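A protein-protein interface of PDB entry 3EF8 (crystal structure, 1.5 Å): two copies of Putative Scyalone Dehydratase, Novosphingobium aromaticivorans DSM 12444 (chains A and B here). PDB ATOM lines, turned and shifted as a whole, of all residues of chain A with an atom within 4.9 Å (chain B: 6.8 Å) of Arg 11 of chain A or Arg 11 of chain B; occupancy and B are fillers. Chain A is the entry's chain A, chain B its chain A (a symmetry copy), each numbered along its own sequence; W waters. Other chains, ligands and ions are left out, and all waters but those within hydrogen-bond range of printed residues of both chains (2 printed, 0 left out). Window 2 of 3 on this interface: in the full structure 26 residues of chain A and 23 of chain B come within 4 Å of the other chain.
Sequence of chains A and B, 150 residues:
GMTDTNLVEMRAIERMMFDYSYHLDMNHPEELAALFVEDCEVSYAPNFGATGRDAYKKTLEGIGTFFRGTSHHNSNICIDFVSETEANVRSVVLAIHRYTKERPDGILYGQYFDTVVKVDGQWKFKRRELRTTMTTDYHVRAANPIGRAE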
ATOM      1  N   LEU A   7     -20.373  21.313 -29.702  1.00  0.00           N
ATOM      2  CA  LEU A   7     -20.318  22.732 -29.321  1.00  0.00           C
ATOM      3  C   LEU A   7     -21.061  23.648 -30.270  1.00  0.00           C
ATOM      4  O   LEU A   7     -21.799  24.586 -29.885  1.00  0.00           O
ATOM      5  CB  LEU A   7     -18.877  23.204 -29.148  1.00  0.00           C
ATOM      6  CG  LEU A   7     -18.119  22.561 -28.002  1.00  0.00           C
ATOM      7  CD1 LEU A   7     -16.667  23.012 -28.061  1.00  0.00           C
ATOM      8  CD2 LEU A   7     -18.682  22.876 -26.625  1.00  0.00           C
ATOM      9  N   VAL A   8     -20.896  23.421 -31.558  1.00  0.00           N
ATOM     10  CA  VAL A   8     -21.545  24.238 -32.533  1.00  0.00           C
ATOM     11  C   VAL A   8     -23.045  24.038 -32.454  1.00  0.00           C
ATOM     12  O   VAL A   8     -23.824  25.002 -32.521  1.00  0.00           O
ATOM     13  CB  VAL A   8     -21.061  23.851 -33.955  1.00  0.00           C
ATOM     14  CG1 VAL A   8     -21.996  24.375 -34.991  1.00  0.00           C
ATOM     15  CG2 VAL A   8     -19.616  24.378 -34.146  1.00  0.00           C
ATOM     16  N   GLU A   9     -23.473  22.792 -32.295  1.00  0.00           N
ATOM     17  CA  GLU A   9     -24.917  22.517 -32.295  1.00  0.00           C
ATOM     18  C   GLU A   9     -25.586  23.008 -30.999  1.00  0.00           C
ATOM     19  O   GLU A   9     -26.760  23.359 -31.005  1.00  0.00           O
ATOM     20  CB  GLU A   9     -25.213  21.051 -32.494  1.00  0.00           C
ATOM     21  CG  GLU A   9     -24.732  20.503 -33.847  1.00  0.00           C
ATOM     22  CD  GLU A   9     -25.302  21.164 -35.081  1.00  0.00           C
ATOM     23  OE1 GLU A   9     -26.050  22.158 -34.997  1.00  0.00           O
ATOM     24  OE2 GLU A   9     -25.033  20.654 -36.216  1.00  0.00           O
ATOM     25  N   MET A  10     -24.831  23.054 -29.904  1.00  0.00           N
ATOM     26  CA  MET A  10     -25.384  23.627 -28.655  1.00  0.00           C
ATOM     27  C   MET A  10     -25.725  25.082 -28.907  1.00  0.00           C
ATOM     28  O   MET A  10     -26.809  25.572 -28.541  1.00  0.00           O
ATOM     29  CB  MET A  10     -24.428  23.494 -27.494  1.00  0.00           C
ATOM     30  CG  MET A  10     -24.388  22.109 -26.988  1.00  0.00           C
ATOM     31  SD  MET A  10     -23.161  21.958 -25.481  1.00  0.00           S
ATOM     32  CE  MET A  10     -24.423  22.784 -24.307  1.00  0.00           C
ATOM     33  N   ARG A  11     -24.820  25.793 -29.561  1.00  0.00           N
ATOM     34  CA  ARG A  11     -25.082  27.182 -29.910  1.00  0.00           C
ATOM     35  C   ARG A  11     -26.283  27.322 -30.817  1.00  0.00           C
ATOM     36  O   ARG A  11     -27.118  28.227 -30.680  1.00  0.00           O
ATOM     37  CB  ARG A  11     -23.850  27.872 -30.531  1.00  0.00           C
ATOM     38  CG  ARG A  11     -22.778  28.189 -29.539  1.00  0.00           C
ATOM     39  CD  ARG A  11     -23.189  29.276 -28.568  1.00  0.00           C
ATOM     40  NE  ARG A  11     -22.087  29.704 -27.784  1.00  0.00           N
ATOM     41  CZ  ARG A  11     -22.153  30.648 -26.893  1.00  0.00           C
ATOM     42  NH1 ARG A  11     -23.355  31.121 -26.638  1.00  0.00           N
ATOM     43  NH2 ARG A  11     -21.106  31.034 -26.219  1.00  0.00           N
ATOM     44  N   ALA A  12     -26.403  26.436 -31.815  1.00  0.00           N
ATOM     45  CA  ALA A  12     -27.526  26.513 -32.736  1.00  0.00           C
ATOM     46  C   ALA A  12     -28.871  26.223 -32.095  1.00  0.00           C
ATOM     47  O   ALA A  12     -29.892  26.863 -32.416  1.00  0.00           O
ATOM     48  CB  ALA A  12     -27.303  25.556 -33.979  1.00  0.00           C
ATOM     49  N   ILE A  13     -28.882  25.253 -31.194  1.00  0.00           N
ATOM     50  CA  ILE A  13     -30.095  24.875 -30.468  1.00  0.00           C
ATOM     51  C   ILE A  13     -30.520  26.064 -29.585  1.00  0.00           C
ATOM     52  O   ILE A  13     -31.683  26.453 -29.560  1.00  0.00           O
ATOM     53  CB  ILE A  13     -29.899  23.573 -29.647  1.00  0.00           C
ATOM     54  CG1 ILE A  13     -29.802  22.391 -30.627  1.00  0.00           C
ATOM     55  CG2 ILE A  13     -31.030  23.408 -28.592  1.00  0.00           C
ATOM     56  CD1 ILE A  13     -29.221  21.161 -29.941  1.00  0.00           C
ATOM     57  N   GLU A  14     -29.561  26.617 -28.853  1.00  0.00           N
ATOM     58  CA  GLU A  14     -29.878  27.761 -27.969  1.00  0.00           C
ATOM     59  C   GLU A  14     -30.408  28.907 -28.823  1.00  0.00           C
ATOM     60  O   GLU A  14     -31.440  29.533 -28.467  1.00  0.00           O
ATOM     61  CB  GLU A  14     -28.642  28.193 -27.217  1.00  0.00           C
ATOM     62  CG  GLU A  14     -28.241  27.240 -26.102  1.00  0.00           C
ATOM     63  CD  GLU A  14     -26.943  27.505 -25.432  1.00  0.00           C
ATOM     64  OE1 GLU A  14     -26.091  28.197 -26.019  1.00  0.00           O
ATOM     65  OE2 GLU A  14     -26.748  26.947 -24.314  1.00  0.00           O
ATOM     66  N   ARG A  15     -29.740  29.213 -29.939  1.00  0.00           N
ATOM     67  CA  ARG A  15     -30.217  30.255 -30.841  1.00  0.00           C
ATOM     68  C   ARG A  15     -31.667  30.028 -31.274  1.00  0.00           C
ATOM     69  O   ARG A  15     -32.477  30.975 -31.328  1.00  0.00           O
ATOM     70  CB  ARG A  15     -29.283  30.380 -32.067  1.00  0.00           C
ATOM     71  CG  ARG A  15     -29.714  31.355 -33.120  1.00  0.00           C
ATOM     72  CD  ARG A  15     -30.020  32.735 -32.531  1.00  0.00           C
ATOM     73  NE  ARG A  15     -30.310  33.716 -33.568  1.00  0.00           N
ATOM     74  CZ  ARG A  15     -29.388  34.387 -34.256  1.00  0.00           C
ATOM     75  NH1 ARG A  15     -28.089  34.233 -34.034  1.00  0.00           N
ATOM     76  NH2 ARG A  15     -29.808  35.228 -35.188  1.00  0.00           N
ATOM     77  N   ASN B   6     -10.930  24.664 -22.781  1.00  0.00           N
ATOM     78  CA  ASN B   6     -11.659  25.740 -22.113  1.00  0.00           C
ATOM     79  C   ASN B   6     -13.125  25.739 -22.543  1.00  0.00           C
ATOM     80  O   ASN B   6     -14.016  25.809 -21.702  1.00  0.00           O
ATOM     81  CB  ASN B   6     -10.994  27.083 -22.296  1.00  0.00           C
ATOM     82  CG  ASN B   6      -9.730  27.205 -21.455  1.00  0.00           C
ATOM     83  OD1 ASN B   6      -9.294  26.227 -20.842  1.00  0.00           O
ATOM     84  ND2 ASN B   6      -9.160  28.388 -21.404  1.00  0.00           N
ATOM     85  N   LEU B   7     -13.391  25.600 -23.829  1.00  0.00           N
ATOM     86  CA  LEU B   7     -14.785  25.649 -24.292  1.00  0.00           C
ATOM     87  C   LEU B   7     -15.638  24.508 -23.782  1.00  0.00           C
ATOM     88  O   LEU B   7     -16.806  24.659 -23.352  1.00  0.00           O
ATOM     89  CB  LEU B   7     -14.861  25.727 -25.815  1.00  0.00           C
ATOM     90  CG  LEU B   7     -14.303  26.999 -26.426  1.00  0.00           C
ATOM     91  CD1 LEU B   7     -14.305  26.856 -27.941  1.00  0.00           C
ATOM     92  CD2 LEU B   7     -15.060  28.261 -26.044  1.00  0.00           C
ATOM     93  N   VAL B   8     -15.094  23.307 -23.811  1.00  0.00           N
ATOM     94  CA  VAL B   8     -15.822  22.163 -23.362  1.00  0.00           C
ATOM     95  C   VAL B   8     -16.073  22.268 -21.871  1.00  0.00           C
ATOM     96  O   VAL B   8     -17.177  21.973 -21.385  1.00  0.00           O
ATOM     97  CB  VAL B   8     -15.010  20.873 -23.645  1.00  0.00           C
ATOM     98  CG1 VAL B   8     -15.531  19.734 -22.838  1.00  0.00           C
ATOM     99  CG2 VAL B   8     -15.055  20.584 -25.168  1.00  0.00           C
ATOM    100  N   GLU B   9     -15.065  22.701 -21.126  1.00  0.00           N
ATOM    101  CA  GLU B   9     -15.212  22.746 -19.664  1.00  0.00           C
ATOM    102  C   GLU B   9     -16.145  23.887 -19.225  1.00  0.00           C
ATOM    103  O   GLU B   9     -16.801  23.787 -18.193  1.00  0.00           O
ATOM    104  CB  GLU B   9     -13.882  22.882 -18.966  1.00  0.00           C
ATOM    105  CG  GLU B   9     -12.934  21.695 -19.206  1.00  0.00           C
ATOM    106  CD  GLU B   9     -13.438  20.336 -18.776  1.00  0.00           C
ATOM    107  OE1 GLU B   9     -14.594  20.183 -18.336  1.00  0.00           O
ATOM    108  OE2 GLU B   9     -12.634  19.351 -18.834  1.00  0.00           O
ATOM    109  N   MET B  10     -16.220  24.953 -20.020  1.00  0.00           N
ATOM    110  CA  MET B  10     -17.187  26.031 -19.711  1.00  0.00           C
ATOM    111  C   MET B  10     -18.586  25.451 -19.771  1.00  0.00           C
ATOM    112  O   MET B  10     -19.429  25.682 -18.885  1.00  0.00           O
ATOM    113  CB  MET B  10     -17.054  27.204 -20.654  1.00  0.00           C
ATOM    114  CG  MET B  10     -15.861  28.013 -20.337  1.00  0.00           C
ATOM    115  SD  MET B  10     -15.710  29.530 -21.552  1.00  0.00           S
ATOM    116  CE  MET B  10     -17.096  30.468 -20.628  1.00  0.00           C
ATOM    117  N   ARG B  11     -18.851  24.662 -20.802  1.00  0.00           N
ATOM    118  CA  ARG B  11     -20.145  24.003 -20.914  1.00  0.00           C
ATOM    119  C   ARG B  11     -20.411  23.075 -19.753  1.00  0.00           C
ATOM    120  O   ARG B  11     -21.520  22.991 -19.208  1.00  0.00           O
ATOM    121  CB  ARG B  11     -20.307  23.257 -22.255  1.00  0.00           C
ATOM    122  CG  ARG B  11     -20.523  24.164 -23.423  1.00  0.00           C
ATOM    123  CD  ARG B  11     -21.869  24.857 -23.378  1.00  0.00           C
ATOM    124  NE  ARG B  11     -22.134  25.536 -24.596  1.00  0.00           N
ATOM    125  CZ  ARG B  11     -23.232  26.188 -24.838  1.00  0.00           C
ATOM    126  NH1 ARG B  11     -24.067  26.314 -23.828  1.00  0.00           N
ATOM    127  NH2 ARG B  11     -23.449  26.769 -25.985  1.00  0.00           N
ATOM    128  N   ALA B  12     -19.395  22.302 -19.342  1.00  0.00           N
ATOM    129  CA  ALA B  12     -19.577  21.374 -18.237  1.00  0.00           C
ATOM    130  C   ALA B  12     -19.825  22.048 -16.900  1.00  0.00           C
ATOM    131  O   ALA B  12     -20.637  21.577 -16.078  1.00  0.00           O
ATOM    132  CB  ALA B  12     -18.345  20.385 -18.122  1.00  0.00           C
ATOM    133  N   ILE B  13     -19.122  23.146 -16.669  1.00  0.00           N
ATOM    134  CA  ILE B  13     -19.270  23.924 -15.438  1.00  0.00           C
ATOM    135  C   ILE B  13     -20.696  24.508 -15.404  1.00  0.00           C
ATOM    136  O   ILE B  13     -21.390  24.429 -14.396  1.00  0.00           O
ATOM    137  CB  ILE B  13     -18.181  25.022 -15.311  1.00  0.00           C
ATOM    138  CG1 ILE B  13     -16.833  24.338 -15.028  1.00  0.00           C
ATOM    139  CG2 ILE B  13     -18.578  26.073 -14.235  1.00  0.00           C
ATOM    140  CD1 ILE B  13     -15.673  25.293 -15.281  1.00  0.00           C
ATOM    141  N   GLU B  14     -21.106  25.106 -16.515  1.00  0.00           N
ATOM    142  CA  GLU B  14     -22.459  25.703 -16.572  1.00  0.00           C
ATOM    143  C   GLU B  14     -23.489  24.604 -16.334  1.00  0.00           C
ATOM    144  O   GLU B  14     -24.441  24.796 -15.534  1.00  0.00           O
ATOM    145  CB  GLU B  14     -22.684  26.352 -17.916  1.00  0.00           C
ATOM    146  CG  GLU B  14     -21.929  27.659 -18.097  1.00  0.00           C
ATOM    147  CD  GLU B  14     -21.961  28.266 -19.451  1.00  0.00           C
ATOM    148  OE1 GLU B  14     -22.239  27.548 -20.430  1.00  0.00           O
ATOM    149  OE2 GLU B  14     -21.634  29.485 -19.543  1.00  0.00           O
ATOM    150  N   ARG B  15     -23.339  23.457 -17.001  1.00  0.00           N
ATOM    151  CA  ARG B  15     -24.246  22.335 -16.783  1.00  0.00           C
ATOM    152  C   ARG B  15     -24.344  21.946 -15.305  1.00  0.00           C
ATOM    153  O   ARG B  15     -25.444  21.668 -14.786  1.00  0.00           O
ATOM    154  CB  ARG B  15     -23.829  21.124 -17.650  1.00  0.00           C
ATOM    155  CG  ARG B  15     -24.626  19.871 -17.449  1.00  0.00           C
ATOM    156  CD  ARG B  15     -26.132  20.126 -17.566  1.00  0.00           C
ATOM    157  NE  ARG B  15     -26.899  18.890 -17.504  1.00  0.00           N
ATOM    158  CZ  ARG B  15     -27.115  18.078 -18.537  1.00  0.00           C
ATOM    159  NH1 ARG B  15     -26.656  18.345 -19.753  1.00  0.00           N
ATOM    160  NH2 ARG B  15     -27.812  16.974 -18.318  1.00  0.00           N
ATOM    161  N   MET B  16     -23.205  21.896 -14.630  1.00  0.00           N
ATOM    162  CA  MET B  16     -23.207  21.508 -13.209  1.00  0.00           C
ATOM    163  C   MET B  16     -23.973  22.532 -12.410  1.00  0.00           C
ATOM    164  O   MET B  16     -24.779  22.178 -11.525  1.00  0.00           O
ATOM    165  CB  MET B  16     -21.766  21.330 -12.716  1.00  0.00           C
ATOM    166  CG  MET B  16     -21.639  20.862 -11.317  1.00  0.00           C
ATOM    167  SD  MET B  16     -21.862  22.229  -9.956  1.00  0.00           S
ATOM    168  CE  MET B  16     -20.040  23.027 -10.114  1.00  0.00           C
ATOM    169  N   PHE B  18     -26.351  24.422 -13.401  1.00  0.00           N
ATOM    170  CA  PHE B  18     -27.761  24.278 -13.730  1.00  0.00           C
ATOM    171  C   PHE B  18     -28.332  23.052 -13.097  1.00  0.00           C
ATOM    172  O   PHE B  18     -29.479  23.047 -12.600  1.00  0.00           O
ATOM    173  CB  PHE B  18     -27.988  24.247 -15.230  1.00  0.00           C
ATOM    174  CG  PHE B  18     -27.494  25.476 -15.959  1.00  0.00           C
ATOM    175  CD1 PHE B  18     -27.411  26.715 -15.320  1.00  0.00           C
ATOM    176  CD2 PHE B  18     -27.126  25.397 -17.291  1.00  0.00           C
ATOM    177  CE1 PHE B  18     -26.941  27.863 -16.006  1.00  0.00           C
ATOM    178  CE2 PHE B  18     -26.685  26.510 -17.978  1.00  0.00           C
ATOM    179  CZ  PHE B  18     -26.568  27.736 -17.341  1.00  0.00           C
ATOM    180  N   ILE B  79     -16.459  32.776 -16.443  1.00  0.00           N
ATOM    181  CA  ILE B  79     -15.555  31.712 -15.991  1.00  0.00           C
ATOM    182  C   ILE B  79     -14.122  32.060 -16.328  1.00  0.00           C
ATOM    183  O   ILE B  79     -13.827  32.345 -17.459  1.00  0.00           O
ATOM    184  CB  ILE B  79     -15.923  30.401 -16.659  1.00  0.00           C
ATOM    185  CG1 ILE B  79     -17.389  30.025 -16.297  1.00  0.00           C
ATOM    186  CG2 ILE B  79     -14.927  29.288 -16.201  1.00  0.00           C
ATOM    187  CD1 ILE B  79     -17.917  28.784 -17.024  1.00  0.00           C
ATOM    188  N   PHE B  81     -10.459  30.271 -15.857  1.00  0.00           N
ATOM    189  CA  PHE B  81      -9.735  29.074 -15.497  1.00  0.00           C
ATOM    190  C   PHE B  81      -8.419  29.366 -14.780  1.00  0.00           C
ATOM    191  O   PHE B  81      -7.627  30.178 -15.266  1.00  0.00           O
ATOM    192  CB  PHE B  81      -9.475  28.202 -16.706  1.00  0.00           C
ATOM    193  CG  PHE B  81     -10.704  27.546 -17.242  1.00  0.00           C
ATOM    194  CD1 PHE B  81     -11.193  26.371 -16.676  1.00  0.00           C
ATOM    195  CD2 PHE B  81     -11.375  28.123 -18.277  1.00  0.00           C
ATOM    196  CE1 PHE B  81     -12.342  25.775 -17.162  1.00  0.00           C
ATOM    197  CE2 PHE B  81     -12.528  27.550 -18.756  1.00  0.00           C
ATOM    198  CZ  PHE B  81     -13.006  26.379 -18.217  1.00  0.00           C
ATOM    199  N   TRP B 123     -17.205  18.279 -12.379  1.00  0.00           N
ATOM    200  CA  TRP B 123     -17.027  19.550 -11.698  1.00  0.00           C
ATOM    201  C   TRP B 123     -17.854  19.591 -10.442  1.00  0.00           C
ATOM    202  O   TRP B 123     -19.004  19.159 -10.411  1.00  0.00           O
ATOM    203  CB  TRP B 123     -17.387  20.725 -12.632  1.00  0.00           C
ATOM    204  CG  TRP B 123     -16.366  20.914 -13.761  1.00  0.00           C
ATOM    205  CD1 TRP B 123     -16.432  20.419 -15.011  1.00  0.00           C
ATOM    206  CD2 TRP B 123     -15.118  21.638 -13.684  1.00  0.00           C
ATOM    207  NE1 TRP B 123     -15.326  20.800 -15.750  1.00  0.00           N
ATOM    208  CE2 TRP B 123     -14.495  21.521 -14.938  1.00  0.00           C
ATOM    209  CE3 TRP B 123     -14.471  22.340 -12.675  1.00  0.00           C
ATOM    210  CZ2 TRP B 123     -13.279  22.135 -15.223  1.00  0.00           C
ATOM    211  CZ3 TRP B 123     -13.255  22.941 -12.968  1.00  0.00           C
ATOM    212  CH2 TRP B 123     -12.683  22.831 -14.221  1.00  0.00           C
HETATM  213  O   HOH W   1     -21.239  25.672 -27.379  1.00  0.00           O
HETATM  214  O   HOH W   2     -26.711  26.726 -21.635  1.00  0.00           O
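CB of Leu 7 of chain B touches CD1 of Leu 7 of chain A (3.96 Å). Leu 7 of chain A touches Arg 11 of chain B. CE of Met 10 of chain A touches CD of Arg 11 of chain B, 3.4 Å away. NH2 of Arg 11 of chain B touches CD of Arg 11 of chain A, at 3.6 Å.
Of chain B, only Arg 11 comes within 4 Å of Arg 11 of chain A. Of chain A, only Leu 7, Met 10, Arg 11 and Glu 14 come within 4 Å of Arg 11 of chain B. Printed residues of chain A within 4 Å of Leu 7 of chain B: Leu 7. Of the printed residues of chain B, Leu 7 of chain A touches Leu 7 and Arg 11. Glu 14 of chain B touches none of the printed residues of chain A. Phe 81 of chain B touches none of the printed residues of chain A. The nearest residue of chain B that does not touch Arg 11 of chain A is Leu 7 of chain B (6.7 Å). The nearest printed residue of chain B that does not touch Glu 14 of chain A is Glu 14 of chain B (6.0 Å).
The side-chain carboxylate (OE2) of Glu 14 of chain A lies within salt-bridge range of the guanidinium group (NH1) of Arg 11 of chain B (2.8 Å).
Water W2 bridges OE2 of Glu 14 of chain A (2.7 Å) and NH1 of Arg 11 of chain B (3.5 Å). Water W1 bridges the backbone carbonyl oxygen of Leu 7 of chain A and the guanidinium group of Arg 11 of chain B.
Leu 7 of chain A touches its own counterpart, Leu 7 of chain B. Leu 7 of chain A touches Arg 11 of chain B, but with the chains exchanged Arg 11 of chain A does not touch Leu 7 of chain B (6.7 Å). Met 10 of chain A touches Arg 11 of chain B, but with the chains exchanged Arg 11 of chain A does not touch Met 10 of chain B (6.9 Å). Glu 14 of chain A touches Arg 11 of chain B, but with the chains exchanged Arg 11 of chain A does not touch Glu 14 of chain B (6.9 Å). 9 positions are printed for both chains. Of the 5 pairs that touch across the chains among the printed residues, 2 have their exchanged pair printed and touching as well.
Along chain B the printed residues that touch a printed residue of chain A span positions 7 to 11. Printed residues of chain A that touch a printed residue of chain B: Leu 7, Met 10, Arg 11 and Glu 14. Hydrophobic or aromatic side chains of chain A that line the printed part of chain B: Leu 7 and Met 10. Among the printed residues, 5 pairs touch across the chains.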
